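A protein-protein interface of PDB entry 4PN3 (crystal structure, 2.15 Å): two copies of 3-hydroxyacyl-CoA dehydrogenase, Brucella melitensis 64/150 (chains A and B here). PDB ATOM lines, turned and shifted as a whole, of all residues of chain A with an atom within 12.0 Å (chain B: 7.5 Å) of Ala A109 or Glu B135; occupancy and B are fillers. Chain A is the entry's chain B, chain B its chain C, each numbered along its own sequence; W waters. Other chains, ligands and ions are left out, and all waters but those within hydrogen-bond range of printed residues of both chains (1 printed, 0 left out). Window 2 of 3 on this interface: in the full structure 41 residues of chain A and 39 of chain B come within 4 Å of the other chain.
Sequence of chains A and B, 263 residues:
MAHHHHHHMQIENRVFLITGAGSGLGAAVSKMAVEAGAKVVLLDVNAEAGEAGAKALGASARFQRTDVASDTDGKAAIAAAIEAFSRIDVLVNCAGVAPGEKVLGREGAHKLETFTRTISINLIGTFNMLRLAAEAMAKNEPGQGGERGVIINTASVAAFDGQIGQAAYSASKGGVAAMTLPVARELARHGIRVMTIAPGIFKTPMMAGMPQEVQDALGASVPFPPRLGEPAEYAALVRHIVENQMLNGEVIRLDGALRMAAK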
ATOM      1  N   GLY A 100     -14.806  32.949  28.133  1.00  0.00           N
ATOM      2  CA  GLY A 100     -14.150  32.655  26.855  1.00  0.00           C
ATOM      3  C   GLY A 100     -14.340  31.176  26.605  1.00  0.00           C
ATOM      4  O   GLY A 100     -14.072  30.360  27.474  1.00  0.00           O
ATOM      5  N   GLU A 101     -14.832  30.825  25.421  1.00  0.00           N
ATOM      6  CA  GLU A 101     -15.008  29.422  25.046  1.00  0.00           C
ATOM      7  C   GLU A 101     -15.019  29.353  23.523  1.00  0.00           C
ATOM      8  O   GLU A 101     -15.751  30.100  22.850  1.00  0.00           O
ATOM      9  CB  GLU A 101     -16.286  28.809  25.665  1.00  0.00           C
ATOM     10  CG  GLU A 101     -16.464  27.300  25.396  1.00  0.00           C
ATOM     11  CD  GLU A 101     -17.718  26.682  26.038  1.00  0.00           C
ATOM     12  OE1 GLU A 101     -18.360  27.353  26.870  1.00  0.00           O
ATOM     13  OE2 GLU A 101     -18.061  25.515  25.725  1.00  0.00           O
ATOM     14  N   LYS A 102     -14.164  28.498  22.977  1.00  0.00           N
ATOM     15  CA  LYS A 102     -14.070  28.376  21.539  1.00  0.00           C
ATOM     16  C   LYS A 102     -15.261  27.637  20.975  1.00  0.00           C
ATOM     17  O   LYS A 102     -15.890  26.840  21.650  1.00  0.00           O
ATOM     18  CB  LYS A 102     -12.805  27.641  21.136  1.00  0.00           C
ATOM     19  CG  LYS A 102     -11.569  28.497  21.326  1.00  0.00           C
ATOM     20  CD  LYS A 102     -10.303  27.704  21.149  1.00  0.00           C
ATOM     21  CE  LYS A 102      -9.108  28.623  20.987  1.00  0.00           C
ATOM     22  NZ  LYS A 102      -8.030  27.857  20.328  1.00  0.00           N
ATOM     23  N   VAL A 103     -15.567  27.974  19.727  1.00  0.00           N
ATOM     24  CA  VAL A 103     -16.578  27.299  18.958  1.00  0.00           C
ATOM     25  C   VAL A 103     -16.170  25.851  18.797  1.00  0.00           C
ATOM     26  O   VAL A 103     -16.991  24.973  19.021  1.00  0.00           O
ATOM     27  CB  VAL A 103     -16.772  27.973  17.585  1.00  0.00           C
ATOM     28  CG1 VAL A 103     -17.720  27.182  16.694  1.00  0.00           C
ATOM     29  CG2 VAL A 103     -17.294  29.390  17.765  1.00  0.00           C
ATOM     30  N   LEU A 104     -14.914  25.620  18.424  1.00  0.00           N
ATOM     31  CA  LEU A 104     -14.334  24.286  18.360  1.00  0.00           C
ATOM     32  C   LEU A 104     -13.170  24.188  19.340  1.00  0.00           C
ATOM     33  O   LEU A 104     -12.064  24.671  19.050  1.00  0.00           O
ATOM     34  CB  LEU A 104     -13.868  23.946  16.936  1.00  0.00           C
ATOM     35  CG  LEU A 104     -14.934  24.016  15.837  1.00  0.00           C
ATOM     36  CD1 LEU A 104     -14.333  23.693  14.478  1.00  0.00           C
ATOM     37  CD2 LEU A 104     -16.121  23.108  16.129  1.00  0.00           C
ATOM     38  N   GLY A 105     -13.418  23.554  20.484  1.00  0.00           N
ATOM     39  CA  GLY A 105     -12.431  23.425  21.548  1.00  0.00           C
ATOM     40  C   GLY A 105     -11.752  22.058  21.541  1.00  0.00           C
ATOM     41  O   GLY A 105     -12.089  21.193  20.732  1.00  0.00           O
ATOM     42  N   ARG A 106     -10.801  21.874  22.448  1.00  0.00           N
ATOM     43  CA  ARG A 106     -10.074  20.620  22.580  1.00  0.00           C
ATOM     44  C   ARG A 106     -11.041  19.436  22.804  1.00  0.00           C
ATOM     45  O   ARG A 106     -10.886  18.376  22.188  1.00  0.00           O
ATOM     46  CB  ARG A 106      -9.024  20.722  23.694  1.00  0.00           C
ATOM     47  N   GLU A 107     -12.055  19.641  23.645  1.00  0.00           N
ATOM     48  CA  GLU A 107     -13.034  18.592  23.973  1.00  0.00           C
ATOM     49  C   GLU A 107     -14.337  18.710  23.216  1.00  0.00           C
ATOM     50  O   GLU A 107     -15.366  18.243  23.700  1.00  0.00           O
ATOM     51  CB  GLU A 107     -13.403  18.581  25.455  1.00  0.00           C
ATOM     52  CG  GLU A 107     -12.654  17.575  26.322  1.00  0.00           C
ATOM     53  CD  GLU A 107     -11.147  17.728  26.395  1.00  0.00           C
ATOM     54  OE1 GLU A 107     -10.585  18.808  26.181  1.00  0.00           O
ATOM     55  OE2 GLU A 107     -10.507  16.704  26.682  1.00  0.00           O
ATOM     56  N   GLY A 108     -14.323  19.351  22.064  1.00  0.00           N
ATOM     57  CA  GLY A 108     -15.480  19.337  21.180  1.00  0.00           C
ATOM     58  C   GLY A 108     -16.064  20.727  20.993  1.00  0.00           C
ATOM     59  O   GLY A 108     -15.442  21.737  21.329  1.00  0.00           O
ATOM     60  N   ALA A 109     -17.292  20.760  20.494  1.00  0.00           N
ATOM     61  CA  ALA A 109     -17.988  22.008  20.225  1.00  0.00           C
ATOM     62  C   ALA A 109     -18.310  22.786  21.510  1.00  0.00           C
ATOM     63  O   ALA A 109     -18.516  22.190  22.568  1.00  0.00           O
ATOM     64  CB  ALA A 109     -19.272  21.728  19.447  1.00  0.00           C
ATOM     65  N   HIS A 110     -18.343  24.115  21.398  1.00  0.00           N
ATOM     66  CA  HIS A 110     -18.886  25.006  22.438  1.00  0.00           C
ATOM     67  C   HIS A 110     -20.155  24.376  23.011  1.00  0.00           C
ATOM     68  O   HIS A 110     -21.018  23.981  22.250  1.00  0.00           O
ATOM     69  CB  HIS A 110     -19.253  26.353  21.777  1.00  0.00           C
ATOM     70  CG  HIS A 110     -19.397  27.517  22.714  1.00  0.00           C
ATOM     71  ND1 HIS A 110     -20.316  27.550  23.737  1.00  0.00           N
ATOM     72  CD2 HIS A 110     -18.785  28.731  22.718  1.00  0.00           C
ATOM     73  CE1 HIS A 110     -20.229  28.713  24.365  1.00  0.00           C
ATOM     74  NE2 HIS A 110     -19.311  29.448  23.763  1.00  0.00           N
ATOM     75  N   LYS A 111     -20.283  24.308  24.328  1.00  0.00           N
ATOM     76  CA  LYS A 111     -21.492  23.768  24.927  1.00  0.00           C
ATOM     77  C   LYS A 111     -22.631  24.735  24.664  1.00  0.00           C
ATOM     78  O   LYS A 111     -22.456  25.968  24.749  1.00  0.00           O
ATOM     79  CB  LYS A 111     -21.336  23.552  26.443  1.00  0.00           C
ATOM     80  CG  LYS A 111     -20.569  22.343  26.942  1.00  0.00           C
ATOM     81  CD  LYS A 111     -20.384  22.340  28.465  1.00  0.00           C
ATOM     82  CE  LYS A 111     -19.259  21.378  28.930  1.00  0.00           C
ATOM     83  NZ  LYS A 111     -19.080  20.067  28.209  1.00  0.00           N
ATOM     84  N   LEU A 112     -23.795  24.208  24.340  1.00  0.00           N
ATOM     85  CA  LEU A 112     -24.961  25.045  24.158  1.00  0.00           C
ATOM     86  C   LEU A 112     -25.390  25.712  25.469  1.00  0.00           C
ATOM     87  O   LEU A 112     -25.937  26.828  25.481  1.00  0.00           O
ATOM     88  CB  LEU A 112     -26.128  24.226  23.611  1.00  0.00           C
ATOM     89  CG  LEU A 112     -27.374  24.989  23.138  1.00  0.00           C
ATOM     90  CD1 LEU A 112     -27.016  25.875  21.957  1.00  0.00           C
ATOM     91  CD2 LEU A 112     -28.482  24.010  22.751  1.00  0.00           C
ATOM     92  N   GLU A 113     -25.185  24.992  26.567  1.00  0.00           N
ATOM     93  CA  GLU A 113     -25.637  25.434  27.891  1.00  0.00           C
ATOM     94  C   GLU A 113     -24.896  26.701  28.308  1.00  0.00           C
ATOM     95  O   GLU A 113     -25.482  27.570  28.932  1.00  0.00           O
ATOM     96  CB  GLU A 113     -25.393  24.345  28.944  1.00  0.00           C
ATOM     97  CG  GLU A 113     -26.234  23.078  28.803  1.00  0.00           C
ATOM     98  CD  GLU A 113     -25.761  22.095  27.719  1.00  0.00           C
ATOM     99  OE1 GLU A 113     -24.727  22.309  27.031  1.00  0.00           O
ATOM    100  OE2 GLU A 113     -26.488  21.097  27.526  1.00  0.00           O
ATOM    101  N   THR A 114     -23.607  26.755  28.005  1.00  0.00           N
ATOM    102  CA  THR A 114     -22.776  27.864  28.421  1.00  0.00           C
ATOM    103  C   THR A 114     -23.083  29.098  27.590  1.00  0.00           C
ATOM    104  O   THR A 114     -23.184  30.194  28.131  1.00  0.00           O
ATOM    105  CB  THR A 114     -21.305  27.525  28.278  1.00  0.00           C
ATOM    106  OG1 THR A 114     -21.056  27.126  26.927  1.00  0.00           O
ATOM    107  CG2 THR A 114     -20.921  26.380  29.230  1.00  0.00           C
ATOM    108  N   PHE A 115     -23.316  28.901  26.294  1.00  0.00           N
ATOM    109  CA  PHE A 115     -23.809  29.972  25.427  1.00  0.00           C
ATOM    110  C   PHE A 115     -25.124  30.562  25.989  1.00  0.00           C
ATOM    111  O   PHE A 115     -25.258  31.773  26.189  1.00  0.00           O
ATOM    112  CB  PHE A 115     -24.020  29.452  24.014  1.00  0.00           C
ATOM    113  CG  PHE A 115     -24.364  30.503  23.027  1.00  0.00           C
ATOM    114  CD1 PHE A 115     -23.359  31.193  22.355  1.00  0.00           C
ATOM    115  CD2 PHE A 115     -25.689  30.818  22.738  1.00  0.00           C
ATOM    116  CE1 PHE A 115     -23.662  32.165  21.427  1.00  0.00           C
ATOM    117  CE2 PHE A 115     -25.995  31.815  21.810  1.00  0.00           C
ATOM    118  CZ  PHE A 115     -24.974  32.481  21.146  1.00  0.00           C
ATOM    119  N   THR A 116     -26.076  29.684  26.235  1.00  0.00           N
ATOM    120  CA  THR A 116     -27.393  30.058  26.711  1.00  0.00           C
ATOM    121  C   THR A 116     -27.315  30.839  28.009  1.00  0.00           C
ATOM    122  O   THR A 116     -27.992  31.843  28.170  1.00  0.00           O
ATOM    123  CB  THR A 116     -28.258  28.783  26.911  1.00  0.00           C
ATOM    124  OG1 THR A 116     -28.411  28.117  25.657  1.00  0.00           O
ATOM    125  CG2 THR A 116     -29.659  29.140  27.487  1.00  0.00           C
ATOM    126  N   GLY A 165     -12.965  33.044  20.823  1.00  0.00           N
ATOM    127  CA  GLY A 165     -13.515  32.574  22.108  1.00  0.00           C
ATOM    128  C   GLY A 165     -14.662  33.415  22.678  1.00  0.00           C
ATOM    129  O   GLY A 165     -15.240  33.066  23.732  1.00  0.00           O
ATOM    130  N   ALA A 167     -17.675  34.281  21.136  1.00  0.00           N
ATOM    131  CA  ALA A 167     -18.948  34.227  20.436  1.00  0.00           C
ATOM    132  C   ALA A 167     -20.100  34.563  21.386  1.00  0.00           C
ATOM    133  O   ALA A 167     -20.956  35.407  21.067  1.00  0.00           O
ATOM    134  CB  ALA A 167     -19.164  32.871  19.799  1.00  0.00           C
ATOM    135  N   ALA A 168     -20.136  33.918  22.539  1.00  0.00           N
ATOM    136  CA  ALA A 168     -21.272  34.077  23.454  1.00  0.00           C
ATOM    137  C   ALA A 168     -21.320  35.493  23.986  1.00  0.00           C
ATOM    138  O   ALA A 168     -22.347  36.139  23.928  1.00  0.00           O
ATOM    139  CB  ALA A 168     -21.161  33.102  24.613  1.00  0.00           C
ATOM    140  N   ILE B  78     -27.140  17.030  11.547  1.00  0.00           N
ATOM    141  CA  ILE B  78     -25.798  16.824  11.034  1.00  0.00           C
ATOM    142  C   ILE B  78     -25.667  15.375  10.572  1.00  0.00           C
ATOM    143  O   ILE B  78     -25.328  15.108   9.426  1.00  0.00           O
ATOM    144  CB  ILE B  78     -24.737  17.107  12.109  1.00  0.00           C
ATOM    145  CG1 ILE B  78     -24.745  18.585  12.531  1.00  0.00           C
ATOM    146  CG2 ILE B  78     -23.361  16.666  11.630  1.00  0.00           C
ATOM    147  CD1 ILE B  78     -24.561  19.599  11.422  1.00  0.00           C
ATOM    148  N   PHE B 127     -26.649  29.954  16.581  1.00  0.00           N
ATOM    149  CA  PHE B 127     -25.412  29.498  17.175  1.00  0.00           C
ATOM    150  C   PHE B 127     -25.334  27.980  17.236  1.00  0.00           C
ATOM    151  O   PHE B 127     -24.313  27.396  16.898  1.00  0.00           O
ATOM    152  CB  PHE B 127     -25.197  30.054  18.573  1.00  0.00           C
ATOM    153  CG  PHE B 127     -23.897  29.625  19.174  1.00  0.00           C
ATOM    154  CD1 PHE B 127     -22.690  30.132  18.672  1.00  0.00           C
ATOM    155  CD2 PHE B 127     -23.847  28.696  20.215  1.00  0.00           C
ATOM    156  CE1 PHE B 127     -21.464  29.716  19.182  1.00  0.00           C
ATOM    157  CE2 PHE B 127     -22.611  28.288  20.737  1.00  0.00           C
ATOM    158  CZ  PHE B 127     -21.428  28.798  20.223  1.00  0.00           C
ATOM    159  N   ASN B 128     -26.429  27.316  17.616  1.00  0.00           N
ATOM    160  CA  ASN B 128     -26.454  25.867  17.708  1.00  0.00           C
ATOM    161  C   ASN B 128     -26.107  25.166  16.374  1.00  0.00           C
ATOM    162  O   ASN B 128     -25.260  24.265  16.331  1.00  0.00           O
ATOM    163  CB  ASN B 128     -27.811  25.389  18.214  1.00  0.00           C
ATOM    164  CG  ASN B 128     -27.851  23.881  18.478  1.00  0.00           C
ATOM    165  OD1 ASN B 128     -27.010  23.348  19.194  1.00  0.00           O
ATOM    166  ND2 ASN B 128     -28.873  23.209  17.959  1.00  0.00           N
ATOM    167  N   MET B 129     -26.751  25.571  15.293  1.00  0.00           N
ATOM    168  CA  MET B 129     -26.476  24.960  14.010  1.00  0.00           C
ATOM    169  C   MET B 129     -25.084  25.313  13.534  1.00  0.00           C
ATOM    170  O   MET B 129     -24.410  24.512  12.915  1.00  0.00           O
ATOM    171  CB  MET B 129     -27.526  25.371  12.983  1.00  0.00           C
ATOM    172  CG  MET B 129     -28.911  24.861  13.301  1.00  0.00           C
ATOM    173  SD  MET B 129     -28.934  23.095  13.761  1.00  0.00           S
ATOM    174  CE  MET B 129     -28.180  22.334  12.319  1.00  0.00           C
ATOM    175  N   LEU B 130     -24.641  26.522  13.861  1.00  0.00           N
ATOM    176  CA  LEU B 130     -23.311  26.979  13.489  1.00  0.00           C
ATOM    177  C   LEU B 130     -22.197  26.138  14.125  1.00  0.00           C
ATOM    178  O   LEU B 130     -21.292  25.673  13.431  1.00  0.00           O
ATOM    179  CB  LEU B 130     -23.199  28.442  13.882  1.00  0.00           C
ATOM    180  CG  LEU B 130     -21.950  29.287  13.809  1.00  0.00           C
ATOM    181  CD1 LEU B 130     -22.397  30.712  14.039  1.00  0.00           C
ATOM    182  CD2 LEU B 130     -20.915  28.908  14.849  1.00  0.00           C
ATOM    183  N   ARG B 131     -22.257  25.981  15.443  1.00  0.00           N
ATOM    184  CA  ARG B 131     -21.274  25.197  16.165  1.00  0.00           C
ATOM    185  C   ARG B 131     -21.175  23.751  15.627  1.00  0.00           C
ATOM    186  O   ARG B 131     -20.071  23.221  15.503  1.00  0.00           O
ATOM    187  CB  ARG B 131     -21.563  25.180  17.675  1.00  0.00           C
ATOM    188  CG  ARG B 131     -22.820  24.407  18.048  1.00  0.00           C
ATOM    189  CD  ARG B 131     -23.431  24.720  19.407  1.00  0.00           C
ATOM    190  NE  ARG B 131     -22.996  23.738  20.374  1.00  0.00           N
ATOM    191  CZ  ARG B 131     -23.583  22.585  20.692  1.00  0.00           C
ATOM    192  NH1 ARG B 131     -24.740  22.163  20.209  1.00  0.00           N
ATOM    193  NH2 ARG B 131     -22.957  21.845  21.557  1.00  0.00           N
ATOM    194  N   LEU B 132     -22.314  23.137  15.312  1.00  0.00           N
ATOM    195  CA  LEU B 132     -22.353  21.755  14.885  1.00  0.00           C
ATOM    196  C   LEU B 132     -21.958  21.581  13.417  1.00  0.00           C
ATOM    197  O   LEU B 132     -21.252  20.627  13.052  1.00  0.00           O
ATOM    198  CB  LEU B 132     -23.749  21.183  15.110  1.00  0.00           C
ATOM    199  CG  LEU B 132     -24.208  21.092  16.575  1.00  0.00           C
ATOM    200  CD1 LEU B 132     -25.670  20.715  16.624  1.00  0.00           C
ATOM    201  CD2 LEU B 132     -23.380  20.087  17.373  1.00  0.00           C
ATOM    202  N   ALA B 133     -22.379  22.515  12.577  1.00  0.00           N
ATOM    203  CA  ALA B 133     -21.933  22.535  11.183  1.00  0.00           C
ATOM    204  C   ALA B 133     -20.434  22.725  11.094  1.00  0.00           C
ATOM    205  O   ALA B 133     -19.762  22.039  10.313  1.00  0.00           O
ATOM    206  CB  ALA B 133     -22.653  23.608  10.397  1.00  0.00           C
ATOM    207  N   ALA B 134     -19.915  23.658  11.872  1.00  0.00           N
ATOM    208  CA  ALA B 134     -18.483  23.961  11.871  1.00  0.00           C
ATOM    209  C   ALA B 134     -17.677  22.724  12.225  1.00  0.00           C
ATOM    210  O   ALA B 134     -16.652  22.424  11.596  1.00  0.00           O
ATOM    211  CB  ALA B 134     -18.189  25.063  12.869  1.00  0.00           C
ATOM    212  N   GLU B 135     -18.130  22.028  13.256  1.00  0.00           N
ATOM    213  CA  GLU B 135     -17.470  20.795  13.687  1.00  0.00           C
ATOM    214  C   GLU B 135     -17.410  19.772  12.543  1.00  0.00           C
ATOM    215  O   GLU B 135     -16.361  19.168  12.309  1.00  0.00           O
ATOM    216  CB  GLU B 135     -18.195  20.198  14.891  1.00  0.00           C
ATOM    217  CG  GLU B 135     -17.572  18.927  15.470  1.00  0.00           C
ATOM    218  CD  GLU B 135     -18.329  18.441  16.708  1.00  0.00           C
ATOM    219  OE1 GLU B 135     -19.591  18.465  16.702  1.00  0.00           O
ATOM    220  OE2 GLU B 135     -17.667  18.038  17.685  1.00  0.00           O
ATOM    221  N   ALA B 136     -18.514  19.596  11.826  1.00  0.00           N
ATOM    222  CA  ALA B 136     -18.530  18.695  10.661  1.00  0.00           C
ATOM    223  C   ALA B 136     -17.599  19.195   9.540  1.00  0.00           C
ATOM    224  O   ALA B 136     -16.823  18.431   8.994  1.00  0.00           O
ATOM    225  CB  ALA B 136     -19.958  18.513  10.149  1.00  0.00           C
ATOM    226  N   MET B 137     -17.693  20.481   9.210  1.00  0.00           N
ATOM    227  CA  MET B 137     -16.891  21.082   8.140  1.00  0.00           C
ATOM    228  C   MET B 137     -15.396  20.941   8.376  1.00  0.00           C
ATOM    229  O   MET B 137     -14.620  20.831   7.423  1.00  0.00           O
ATOM    230  CB  MET B 137     -17.214  22.574   8.008  1.00  0.00           C
ATOM    231  CG  MET B 137     -18.549  22.897   7.375  1.00  0.00           C
ATOM    232  SD  MET B 137     -18.948  24.648   7.509  1.00  0.00           S
ATOM    233  CE  MET B 137     -20.604  24.624   6.825  1.00  0.00           C
ATOM    234  N   ALA B 138     -14.985  21.002   9.636  1.00  0.00           N
ATOM    235  CA  ALA B 138     -13.565  20.898   9.971  1.00  0.00           C
ATOM    236  C   ALA B 138     -12.964  19.542   9.601  1.00  0.00           C
ATOM    237  O   ALA B 138     -11.755  19.423   9.434  1.00  0.00           O
ATOM    238  CB  ALA B 138     -13.344  21.208  11.450  1.00  0.00           C
ATOM    239  N   LYS B 139     -13.802  18.520   9.483  1.00  0.00           N
ATOM    240  CA  LYS B 139     -13.364  17.173   9.073  1.00  0.00           C
ATOM    241  C   LYS B 139     -13.160  17.075   7.556  1.00  0.00           C
ATOM    242  O   LYS B 139     -12.543  16.133   7.101  1.00  0.00           O
ATOM    243  CB  LYS B 139     -14.366  16.076   9.540  1.00  0.00           C
ATOM    244  N   ASN B 140     -13.672  18.035   6.777  1.00  0.00           N
ATOM    245  CA  ASN B 140     -13.472  18.021   5.329  1.00  0.00           C
ATOM    246  C   ASN B 140     -11.999  18.182   5.018  1.00  0.00           C
ATOM    247  O   ASN B 140     -11.255  18.772   5.787  1.00  0.00           O
ATOM    248  CB  ASN B 140     -14.222  19.168   4.618  1.00  0.00           C
ATOM    249  CG  ASN B 140     -15.740  19.034   4.689  1.00  0.00           C
ATOM    250  OD1 ASN B 140     -16.297  17.925   4.774  1.00  0.00           O
ATOM    251  ND2 ASN B 140     -16.420  20.163   4.571  1.00  0.00           N
ATOM    252  N   ILE B 151     -20.140  29.443   6.343  1.00  0.00           N
ATOM    253  CA  ILE B 151     -21.351  29.600   7.166  1.00  0.00           C
ATOM    254  C   ILE B 151     -21.946  30.973   6.929  1.00  0.00           C
ATOM    255  O   ILE B 151     -21.244  31.984   7.023  1.00  0.00           O
ATOM    256  CB  ILE B 151     -21.010  29.407   8.643  1.00  0.00           C
ATOM    257  CG1 ILE B 151     -20.610  27.937   8.899  1.00  0.00           C
ATOM    258  CG2 ILE B 151     -22.190  29.803   9.526  1.00  0.00           C
ATOM    259  CD1 ILE B 151     -19.950  27.713  10.243  1.00  0.00           C
ATOM    260  N   LEU B 187     -12.568  30.343  13.234  1.00  0.00           N
ATOM    261  CA  LEU B 187     -12.765  29.302  12.239  1.00  0.00           C
ATOM    262  C   LEU B 187     -11.869  29.491  11.009  1.00  0.00           C
ATOM    263  O   LEU B 187     -11.772  28.585  10.172  1.00  0.00           O
ATOM    264  CB  LEU B 187     -14.237  29.192  11.836  1.00  0.00           C
ATOM    265  CG  LEU B 187     -15.209  28.860  12.968  1.00  0.00           C
ATOM    266  CD1 LEU B 187     -16.581  28.606  12.374  1.00  0.00           C
ATOM    267  CD2 LEU B 187     -14.764  27.655  13.800  1.00  0.00           C
ATOM    268  N   ILE B 192     -12.786  27.879   7.377  1.00  0.00           N
ATOM    269  CA  ILE B 192     -14.233  28.055   7.343  1.00  0.00           C
ATOM    270  C   ILE B 192     -14.565  29.556   7.442  1.00  0.00           C
ATOM    271  O   ILE B 192     -14.199  30.212   8.430  1.00  0.00           O
ATOM    272  CB  ILE B 192     -14.933  27.315   8.500  1.00  0.00           C
ATOM    273  CG1 ILE B 192     -14.703  25.813   8.395  1.00  0.00           C
ATOM    274  CG2 ILE B 192     -16.426  27.625   8.491  1.00  0.00           C
ATOM    275  CD1 ILE B 192     -15.043  25.052   9.669  1.00  0.00           C
HETATM  276  O   HOH W   1     -18.246  18.427  20.062  1.00  0.00           O
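No position is printed for both chains. Of the 9 pairs that touch across the chains among the printed residues, none has its exchanged pair printed and touching as well.
Water W1 bridges the side-chain carboxylate (OE2) of Glu B135 (2.5 Å) and the backbone NH (N) of Ala A109 (2.6 Å).
Ala B134 touches Leu A104 (O to CD1, 3.9 Å). Leu A104 touches Glu B135 (CD2 to CA, 3.6 Å). OE2 of Glu B135 touches N of Ala A109, at 3.9 Å. His A110 touches Phe B127. Leu A112 touches Asn B128 (CD1 to OD1, 3.7 Å). N of Leu A112 touches NH2 of Arg B131 (3.7 Å). Phe A115 touches Phe B127. Ala A167 touches Phe B127.
Hydrophobic or aromatic side chains of chain A within 4 Å of the printed part of chain B: Leu A104, His A110, Leu A112, Phe A115 and Ala A167. Hydrophobic or aromatic side chains of chain B that line the printed part of chain A: Phe B127. Among the printed residues, 9 pairs touch across the chains. Among the printed residues, no Asp or Glu carboxylate lies within 4 Å of a Lys or Arg side-chain nitrogen of the other chain.
The backbone NH of His A110 lies within hydrogen-bond range of the backbone carbonyl oxygen of Val A103 (2.9 Å). A ring nitrogen (ND1) of His A110 lies close to the side-chain hydroxyl (OG1) of Thr A114 (3.3 Å). O of Leu A112 lies within hydrogen-bond range of OG1 of Thr A116 (2.8 Å). The side-chain amide oxygen (OD1) of Asn B128 lies within hydrogen-bond range of the guanidinium group (NH1) of Arg B131.
The guanidinium group (NE) of Arg B131 lies within hydrogen-bond range of the backbone carbonyl oxygen (O) of His A110, at 2.7 Å.
Lys A102 touches none of the printed residues of chain B. Of the printed residues of chain B, Leu A104 touches Ala B134 (3.9 Å) and Glu B135 (3.6 Å). Ala A109 touches just one residue of chain B: Glu B135 (3.9 Å). Of the printed residues of chain B, Leu A112 touches Asn B128 and Arg B131. Printed residues of chain B within 4 Å of Phe A115: Phe B127. Of the printed residues of chain B, Ala A167 touches Phe B127 (3.95 Å). Ile B78 touches none of the printed residues of chain A. Of the printed residues of chain A, Phe B127 touches His A110 (3.5 Å), Phe A115 (3.3 Å) and Ala A167 (3.95 Å). No residue of chain A comes within 4 Å of Leu B132. No residue of chain A comes within 4 Å of Ala B133. Of chain A, only Leu A104 (3.9 Å) comes within 4 Å of Ala B134. No residue of chain A comes within 4 Å of Met B137. No residue of chain A comes within 4 Å of Ala B138. The nearest residue of chain A that does not touch Glu B135 is Gly A108 (4.3 Å).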
